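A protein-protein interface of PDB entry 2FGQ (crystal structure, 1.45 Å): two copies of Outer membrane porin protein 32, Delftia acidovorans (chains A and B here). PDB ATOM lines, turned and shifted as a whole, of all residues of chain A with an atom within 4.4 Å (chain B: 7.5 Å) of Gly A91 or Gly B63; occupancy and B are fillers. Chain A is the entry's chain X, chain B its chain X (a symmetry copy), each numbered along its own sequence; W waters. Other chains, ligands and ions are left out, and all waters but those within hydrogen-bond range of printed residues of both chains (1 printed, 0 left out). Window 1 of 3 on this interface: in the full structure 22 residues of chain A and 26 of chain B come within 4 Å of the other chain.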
ATOM      1  N   SER A  77     -16.073  -9.091  29.981  1.00  0.00           N
ATOM      2  CA  SER A  77     -17.530  -9.092  29.916  1.00  0.00           C
ATOM      3  C   SER A  77     -18.040 -10.217  30.774  1.00  0.00           C
ATOM      4  O   SER A  77     -18.491 -11.240  30.265  1.00  0.00           O
ATOM      5  CB  SER A  77     -18.034  -9.227  28.473  1.00  0.00           C
ATOM      6  OG  SER A  77     -17.562 -10.387  27.820  1.00  0.00           O
ATOM      7  N   THR A  78     -17.947 -10.029  32.086  1.00  0.00           N
ATOM      8  CA  THR A  78     -18.216 -11.113  33.026  1.00  0.00           C
ATOM      9  C   THR A  78     -19.436 -10.878  33.888  1.00  0.00           C
ATOM     10  O   THR A  78     -19.910  -9.760  34.092  1.00  0.00           O
ATOM     11  CB  THR A  78     -17.008 -11.319  33.991  1.00  0.00           C
ATOM     12  OG1 THR A  78     -16.649 -10.053  34.592  1.00  0.00           O
ATOM     13  CG2 THR A  78     -15.787 -11.822  33.225  1.00  0.00           C
ATOM     14  N   ARG A  89     -16.081 -16.272  38.055  1.00  0.00           N
ATOM     15  CA  ARG A  89     -16.490 -15.396  36.934  1.00  0.00           C
ATOM     16  C   ARG A  89     -16.733 -16.192  35.668  1.00  0.00           C
ATOM     17  O   ARG A  89     -15.971 -17.115  35.348  1.00  0.00           O
ATOM     18  CB  ARG A  89     -15.388 -14.429  36.608  1.00  0.00           C
ATOM     19  CG  ARG A  89     -14.900 -13.566  37.693  1.00  0.00           C
ATOM     20  CD  ARG A  89     -13.819 -12.563  37.160  1.00  0.00           C
ATOM     21  NE  ARG A  89     -13.141 -11.902  38.234  1.00  0.00           N
ATOM     22  CZ  ARG A  89     -12.039 -11.199  38.110  1.00  0.00           C
ATOM     23  NH1 ARG A  89     -11.380 -11.076  36.945  1.00  0.00           N
ATOM     24  NH2 ARG A  89     -11.564 -10.621  39.189  1.00  0.00           N
ATOM     25  N   LEU A  90     -17.798 -15.824  34.955  1.00  0.00           N
ATOM     26  CA  LEU A  90     -18.098 -16.362  33.637  1.00  0.00           C
ATOM     27  C   LEU A  90     -18.045 -15.267  32.598  1.00  0.00           C
ATOM     28  O   LEU A  90     -18.737 -14.263  32.761  1.00  0.00           O
ATOM     29  CB  LEU A  90     -19.526 -16.913  33.569  1.00  0.00           C
ATOM     30  CG  LEU A  90     -19.955 -18.283  34.124  1.00  0.00           C
ATOM     31  CD1 LEU A  90     -19.162 -18.854  35.167  1.00  0.00           C
ATOM     32  CD2 LEU A  90     -21.477 -18.422  34.346  1.00  0.00           C
ATOM     33  N   GLY A  91     -17.324 -15.527  31.505  1.00  0.00           N
ATOM     34  CA  GLY A  91     -17.252 -14.596  30.401  1.00  0.00           C
ATOM     35  C   GLY A  91     -15.835 -14.246  29.995  1.00  0.00           C
ATOM     36  O   GLY A  91     -14.825 -14.562  30.676  1.00  0.00           O
ATOM     37  N   ARG A  92     -15.718 -13.558  28.876  1.00  0.00           N
ATOM     38  CA  ARG A  92     -14.428 -13.129  28.394  1.00  0.00           C
ATOM     39  C   ARG A  92     -13.704 -12.241  29.421  1.00  0.00           C
ATOM     40  O   ARG A  92     -14.294 -11.337  30.012  1.00  0.00           O
ATOM     41  CB  ARG A  92     -14.576 -12.344  27.102  1.00  0.00           C
ATOM     42  CG  ARG A  92     -13.161 -11.998  26.551  1.00  0.00           C
ATOM     43  CD  ARG A  92     -13.175 -11.500  25.205  1.00  0.00           C
ATOM     44  NE  ARG A  92     -11.902 -10.957  24.808  1.00  0.00           N
ATOM     45  CZ  ARG A  92     -10.946 -11.641  24.203  1.00  0.00           C
ATOM     46  NH1 ARG A  92     -11.020 -12.959  24.016  1.00  0.00           N
ATOM     47  NH2 ARG A  92      -9.875 -10.995  23.795  1.00  0.00           N
ATOM     48  N   ASP A  93     -12.431 -12.520  29.625  1.00  0.00           N
ATOM     49  CA  ASP A  93     -11.629 -11.787  30.589  1.00  0.00           C
ATOM     50  C   ASP A  93     -10.186 -12.129  30.359  1.00  0.00           C
ATOM     51  O   ASP A  93      -9.844 -13.053  29.590  1.00  0.00           O
ATOM     52  CB  ASP A  93     -12.061 -12.263  31.980  1.00  0.00           C
ATOM     53  CG  ASP A  93     -11.697 -11.331  33.109  1.00  0.00           C
ATOM     54  OD1 ASP A  93     -11.039 -10.245  32.944  1.00  0.00           O
ATOM     55  OD2 ASP A  93     -12.068 -11.660  34.275  1.00  0.00           O
ATOM     56  N   LEU A 137     -14.636 -18.275  28.910  1.00  0.00           N
ATOM     57  CA  LEU A 137     -13.828 -18.524  30.102  1.00  0.00           C
ATOM     58  C   LEU A 137     -14.652 -18.629  31.408  1.00  0.00           C
ATOM     59  O   LEU A 137     -15.577 -17.846  31.660  1.00  0.00           O
ATOM     60  CB  LEU A 137     -12.810 -17.380  30.205  1.00  0.00           C
ATOM     61  CG  LEU A 137     -11.868 -17.434  31.417  1.00  0.00           C
ATOM     62  CD1 LEU A 137     -10.873 -18.599  31.329  1.00  0.00           C
ATOM     63  CD2 LEU A 137     -11.124 -16.125  31.480  1.00  0.00           C
ATOM     64  N   VAL B  10     -26.896  -9.302  32.237  1.00  0.00           N
ATOM     65  CA  VAL B  10     -25.871 -10.238  31.786  1.00  0.00           C
ATOM     66  C   VAL B  10     -26.349 -11.648  32.188  1.00  0.00           C
ATOM     67  O   VAL B  10     -26.487 -11.957  33.375  1.00  0.00           O
ATOM     68  CB  VAL B  10     -24.466  -9.957  32.343  1.00  0.00           C
ATOM     69  CG1 VAL B  10     -23.495 -10.921  31.725  1.00  0.00           C
ATOM     70  CG2 VAL B  10     -24.052  -8.542  32.057  1.00  0.00           C
ATOM     71  N   ASP B  11     -26.603 -12.454  31.183  1.00  0.00           N
ATOM     72  CA  ASP B  11     -27.084 -13.828  31.340  1.00  0.00           C
ATOM     73  C   ASP B  11     -26.083 -14.693  30.573  1.00  0.00           C
ATOM     74  O   ASP B  11     -25.962 -14.591  29.343  1.00  0.00           O
ATOM     75  CB  ASP B  11     -28.503 -13.953  30.788  1.00  0.00           C
ATOM     76  CG  ASP B  11     -29.033 -15.353  30.820  1.00  0.00           C
ATOM     77  OD1 ASP B  11     -28.250 -16.316  30.584  1.00  0.00           O
ATOM     78  OD2 ASP B  11     -30.255 -15.552  31.021  1.00  0.00           O
ATOM     79  N   THR B  12     -25.320 -15.488  31.328  1.00  0.00           N
ATOM     80  CA  THR B  12     -24.269 -16.333  30.776  1.00  0.00           C
ATOM     81  C   THR B  12     -24.412 -17.722  31.363  1.00  0.00           C
ATOM     82  O   THR B  12     -24.781 -17.881  32.529  1.00  0.00           O
ATOM     83  CB  THR B  12     -22.898 -15.690  31.051  1.00  0.00           C
ATOM     84  OG1 THR B  12     -22.867 -14.424  30.409  1.00  0.00           O
ATOM     85  CG2 THR B  12     -21.748 -16.448  30.430  1.00  0.00           C
ATOM     86  N   LEU B  29     -19.468 -22.206  26.684  1.00  0.00           N
ATOM     87  CA  LEU B  29     -19.979 -21.089  27.461  1.00  0.00           C
ATOM     88  C   LEU B  29     -20.866 -20.313  26.489  1.00  0.00           C
ATOM     89  O   LEU B  29     -20.382 -19.861  25.469  1.00  0.00           O
ATOM     90  CB  LEU B  29     -18.853 -20.209  28.015  1.00  0.00           C
ATOM     91  CG  LEU B  29     -19.336 -19.252  29.121  1.00  0.00           C
ATOM     92  CD1 LEU B  29     -19.470 -20.024  30.429  1.00  0.00           C
ATOM     93  CD2 LEU B  29     -18.442 -18.061  29.253  1.00  0.00           C
ATOM     94  N   GLY B  30     -22.126 -20.172  26.798  1.00  0.00           N
ATOM     95  CA  GLY B  30     -23.063 -19.436  25.987  1.00  0.00           C
ATOM     96  C   GLY B  30     -23.757 -18.343  26.767  1.00  0.00           C
ATOM     97  O   GLY B  30     -23.359 -17.959  27.853  1.00  0.00           O
ATOM     98  N   THR B  31     -24.800 -17.780  26.161  1.00  0.00           N
ATOM     99  CA  THR B  31     -25.484 -16.634  26.730  1.00  0.00           C
ATOM    100  C   THR B  31     -26.977 -16.724  26.626  1.00  0.00           C
ATOM    101  O   THR B  31     -27.527 -17.492  25.809  1.00  0.00           O
ATOM    102  CB  THR B  31     -25.008 -15.316  26.051  1.00  0.00           C
ATOM    103  OG1 THR B  31     -25.362 -15.315  24.645  1.00  0.00           O
ATOM    104  CG2 THR B  31     -23.495 -15.120  26.185  1.00  0.00           C
ATOM    105  N   SER B  32     -27.646 -15.914  27.452  1.00  0.00           N
ATOM    106  CA  SER B  32     -29.023 -15.549  27.196  1.00  0.00           C
ATOM    107  C   SER B  32     -29.965 -16.756  27.226  1.00  0.00           C
ATOM    108  O   SER B  32     -30.842 -16.918  26.370  1.00  0.00           O
ATOM    109  CB  SER B  32     -29.080 -14.753  25.893  1.00  0.00           C
ATOM    110  OG  SER B  32     -28.384 -13.530  26.027  1.00  0.00           O
ATOM    111  N   SER B  37     -29.429 -11.138  27.151  1.00  0.00           N
ATOM    112  CA  SER B  37     -28.468 -10.194  27.710  1.00  0.00           C
ATOM    113  C   SER B  37     -28.507  -8.904  26.931  1.00  0.00           C
ATOM    114  O   SER B  37     -28.634  -8.920  25.717  1.00  0.00           O
ATOM    115  CB  SER B  37     -27.041 -10.732  27.660  1.00  0.00           C
ATOM    116  OG  SER B  37     -26.887 -11.960  28.290  1.00  0.00           O
ATOM    117  N   GLU B  60     -27.838  -5.989  22.358  1.00  0.00           N
ATOM    118  CA  GLU B  60     -27.555  -7.288  22.962  1.00  0.00           C
ATOM    119  C   GLU B  60     -26.101  -7.335  23.443  1.00  0.00           C
ATOM    120  O   GLU B  60     -25.185  -6.723  22.877  1.00  0.00           O
ATOM    121  CB  GLU B  60     -27.753  -8.403  21.939  1.00  0.00           C
ATOM    122  CG  GLU B  60     -27.687  -9.802  22.520  1.00  0.00           C
ATOM    123  CD  GLU B  60     -28.234 -10.912  21.644  1.00  0.00           C
ATOM    124  OE1 GLU B  60     -28.845 -10.636  20.580  1.00  0.00           O
ATOM    125  OE2 GLU B  60     -28.102 -12.099  22.089  1.00  0.00           O
ATOM    126  N   ILE B  61     -25.932  -8.052  24.553  1.00  0.00           N
ATOM    127  CA  ILE B  61     -24.633  -8.374  25.122  1.00  0.00           C
ATOM    128  C   ILE B  61     -24.316  -9.836  24.899  1.00  0.00           C
ATOM    129  O   ILE B  61     -25.154 -10.693  25.080  1.00  0.00           O
ATOM    130  CB  ILE B  61     -24.621  -8.013  26.633  1.00  0.00           C
ATOM    131  CG1 ILE B  61     -24.724  -6.499  26.798  1.00  0.00           C
ATOM    132  CG2 ILE B  61     -23.431  -8.617  27.367  1.00  0.00           C
ATOM    133  CD1 ILE B  61     -23.511  -5.731  26.378  1.00  0.00           C
ATOM    134  N   PHE B  62     -23.080 -10.121  24.551  1.00  0.00           N
ATOM    135  CA  PHE B  62     -22.549 -11.454  24.374  1.00  0.00           C
ATOM    136  C   PHE B  62     -21.368 -11.647  25.311  1.00  0.00           C
ATOM    137  O   PHE B  62     -20.219 -11.355  24.947  1.00  0.00           O
ATOM    138  CB  PHE B  62     -22.132 -11.683  22.900  1.00  0.00           C
ATOM    139  CG  PHE B  62     -23.233 -11.446  21.904  1.00  0.00           C
ATOM    140  CD1 PHE B  62     -24.128 -12.463  21.560  1.00  0.00           C
ATOM    141  CD2 PHE B  62     -23.403 -10.210  21.349  1.00  0.00           C
ATOM    142  CE1 PHE B  62     -25.163 -12.240  20.634  1.00  0.00           C
ATOM    143  CE2 PHE B  62     -24.417  -9.968  20.452  1.00  0.00           C
ATOM    144  CZ  PHE B  62     -25.311 -10.986  20.090  1.00  0.00           C
ATOM    145  N   GLY B  63     -21.650 -12.078  26.536  1.00  0.00           N
ATOM    146  CA  GLY B  63     -20.639 -12.129  27.574  1.00  0.00           C
ATOM    147  C   GLY B  63     -19.567 -13.150  27.314  1.00  0.00           C
ATOM    148  O   GLY B  63     -18.453 -12.993  27.793  1.00  0.00           O
ATOM    149  N   ASP B  64     -19.840 -14.166  26.519  1.00  0.00           N
ATOM    150  CA  ASP B  64     -18.820 -15.179  26.235  1.00  0.00           C
ATOM    151  C   ASP B  64     -17.676 -14.698  25.338  1.00  0.00           C
ATOM    152  O   ASP B  64     -16.583 -15.245  25.413  1.00  0.00           O
ATOM    153  CB  ASP B  64     -19.432 -16.477  25.703  1.00  0.00           C
ATOM    154  CG  ASP B  64     -20.224 -16.302  24.407  1.00  0.00           C
ATOM    155  OD1 ASP B  64     -20.720 -15.193  24.064  1.00  0.00           O
ATOM    156  OD2 ASP B  64     -20.327 -17.309  23.648  1.00  0.00           O
ATOM    157  N   ASP B  65     -17.919 -13.669  24.527  1.00  0.00           N
ATOM    158  CA  ASP B  65     -16.901 -13.130  23.645  1.00  0.00           C
ATOM    159  C   ASP B  65     -16.724 -11.627  23.672  1.00  0.00           C
ATOM    160  O   ASP B  65     -16.025 -11.083  22.825  1.00  0.00           O
ATOM    161  CB  ASP B  65     -17.011 -13.685  22.233  1.00  0.00           C
ATOM    162  CG  ASP B  65     -18.127 -13.078  21.426  1.00  0.00           C
ATOM    163  OD1 ASP B  65     -18.760 -12.078  21.819  1.00  0.00           O
ATOM    164  OD2 ASP B  65     -18.379 -13.548  20.301  1.00  0.00           O
ATOM    165  N   GLY B  66     -17.276 -10.971  24.692  1.00  0.00           N
ATOM    166  CA  GLY B  66     -17.097  -9.533  24.818  1.00  0.00           C
ATOM    167  C   GLY B  66     -17.644  -8.729  23.677  1.00  0.00           C
ATOM    168  O   GLY B  66     -17.076  -7.715  23.337  1.00  0.00           O
ATOM    169  N   ASN B  67     -18.744  -9.192  23.090  1.00  0.00           N
ATOM    170  CA  ASN B  67     -19.325  -8.508  21.932  1.00  0.00           C
ATOM    171  C   ASN B  67     -18.252  -8.337  20.850  1.00  0.00           C
ATOM    172  O   ASN B  67     -18.060  -7.258  20.285  1.00  0.00           O
ATOM    173  CB  ASN B  67     -19.953  -7.160  22.295  1.00  0.00           C
ATOM    174  CG  ASN B  67     -21.315  -7.284  22.896  1.00  0.00           C
ATOM    175  OD1 ASN B  67     -21.451  -7.771  24.013  1.00  0.00           O
ATOM    176  ND2 ASN B  67     -22.354  -6.866  22.128  1.00  0.00           N
HETATM  177  O   HOH W   1     -20.462 -13.157  30.935  1.00  0.00           O
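OG of Ser A77 sits at hydrogen-bond distance from O of Gly B63 (2.8 Å).
N of Arg A92 lies within hydrogen-bond range of O of Gly B63, 3.0 Å away.
The side-chain hydroxyl of Ser A77 lies close to the backbone NH of Gly B66, at 3.2 Å.
The backbone carbonyl oxygen of Arg A92 sits at hydrogen-bond distance from the backbone NH of Ser A77 (2.9 Å).
O of Leu A137 lies within hydrogen-bond range of N of Gly A91.
The side-chain carboxylate of Asp B65 is in hydrogen-bond range of the backbone NH of Asn B67.
Among the printed residues, merely in contact across the chains: Gly A91 with Gly B63, Gly A91 with Leu B29, Arg A92 with Asp B65, Leu A137 with Leu B29, Leu A90 with Thr B12, Arg A92 with Gly B66 and Arg A92 with Asp B64.
Of chain B, only Leu B29 (3.6 Å) and Gly B63 (3.3 Å) come within 4 Å of Gly A91.
Gly B63 touches just these residues of chain A: Ser A77 (2.8 Å), Gly A91 (3.3 Å) and Arg A92 (3.0 Å).
Of the printed residues of chain A, Leu B29 touches Gly A91 and Leu A137.
Printed residues of chain B within 4 Å of Ser A77: Gly B63 and Gly B66.
Of the printed residues of chain A, Thr B12 touches Leu A90.
Asn B67 touches none of the printed residues of chain A.
The nearest printed residue of chain A that does not touch Gly B63 is Leu A90 (5.1 Å).
Hydrophobic or aromatic side chains of chain B within 4 Å of the printed part of chain A: Leu B29.
Hydrophobic or aromatic side chains of chain A that line the printed part of chain B: Leu A90.
Among the printed residues, 10 pairs touch across the chains.
No position is printed for both chains.
Of the 10 pairs that touch across the chains among the printed residues, none has its exchanged pair printed and touching as well.
Water W1 lies within hydrogen-bond range of O of Leu A90 (2.7 Å), OG1 of Thr B12 (2.8 Å) and O of Ser A77 (2.8 Å).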
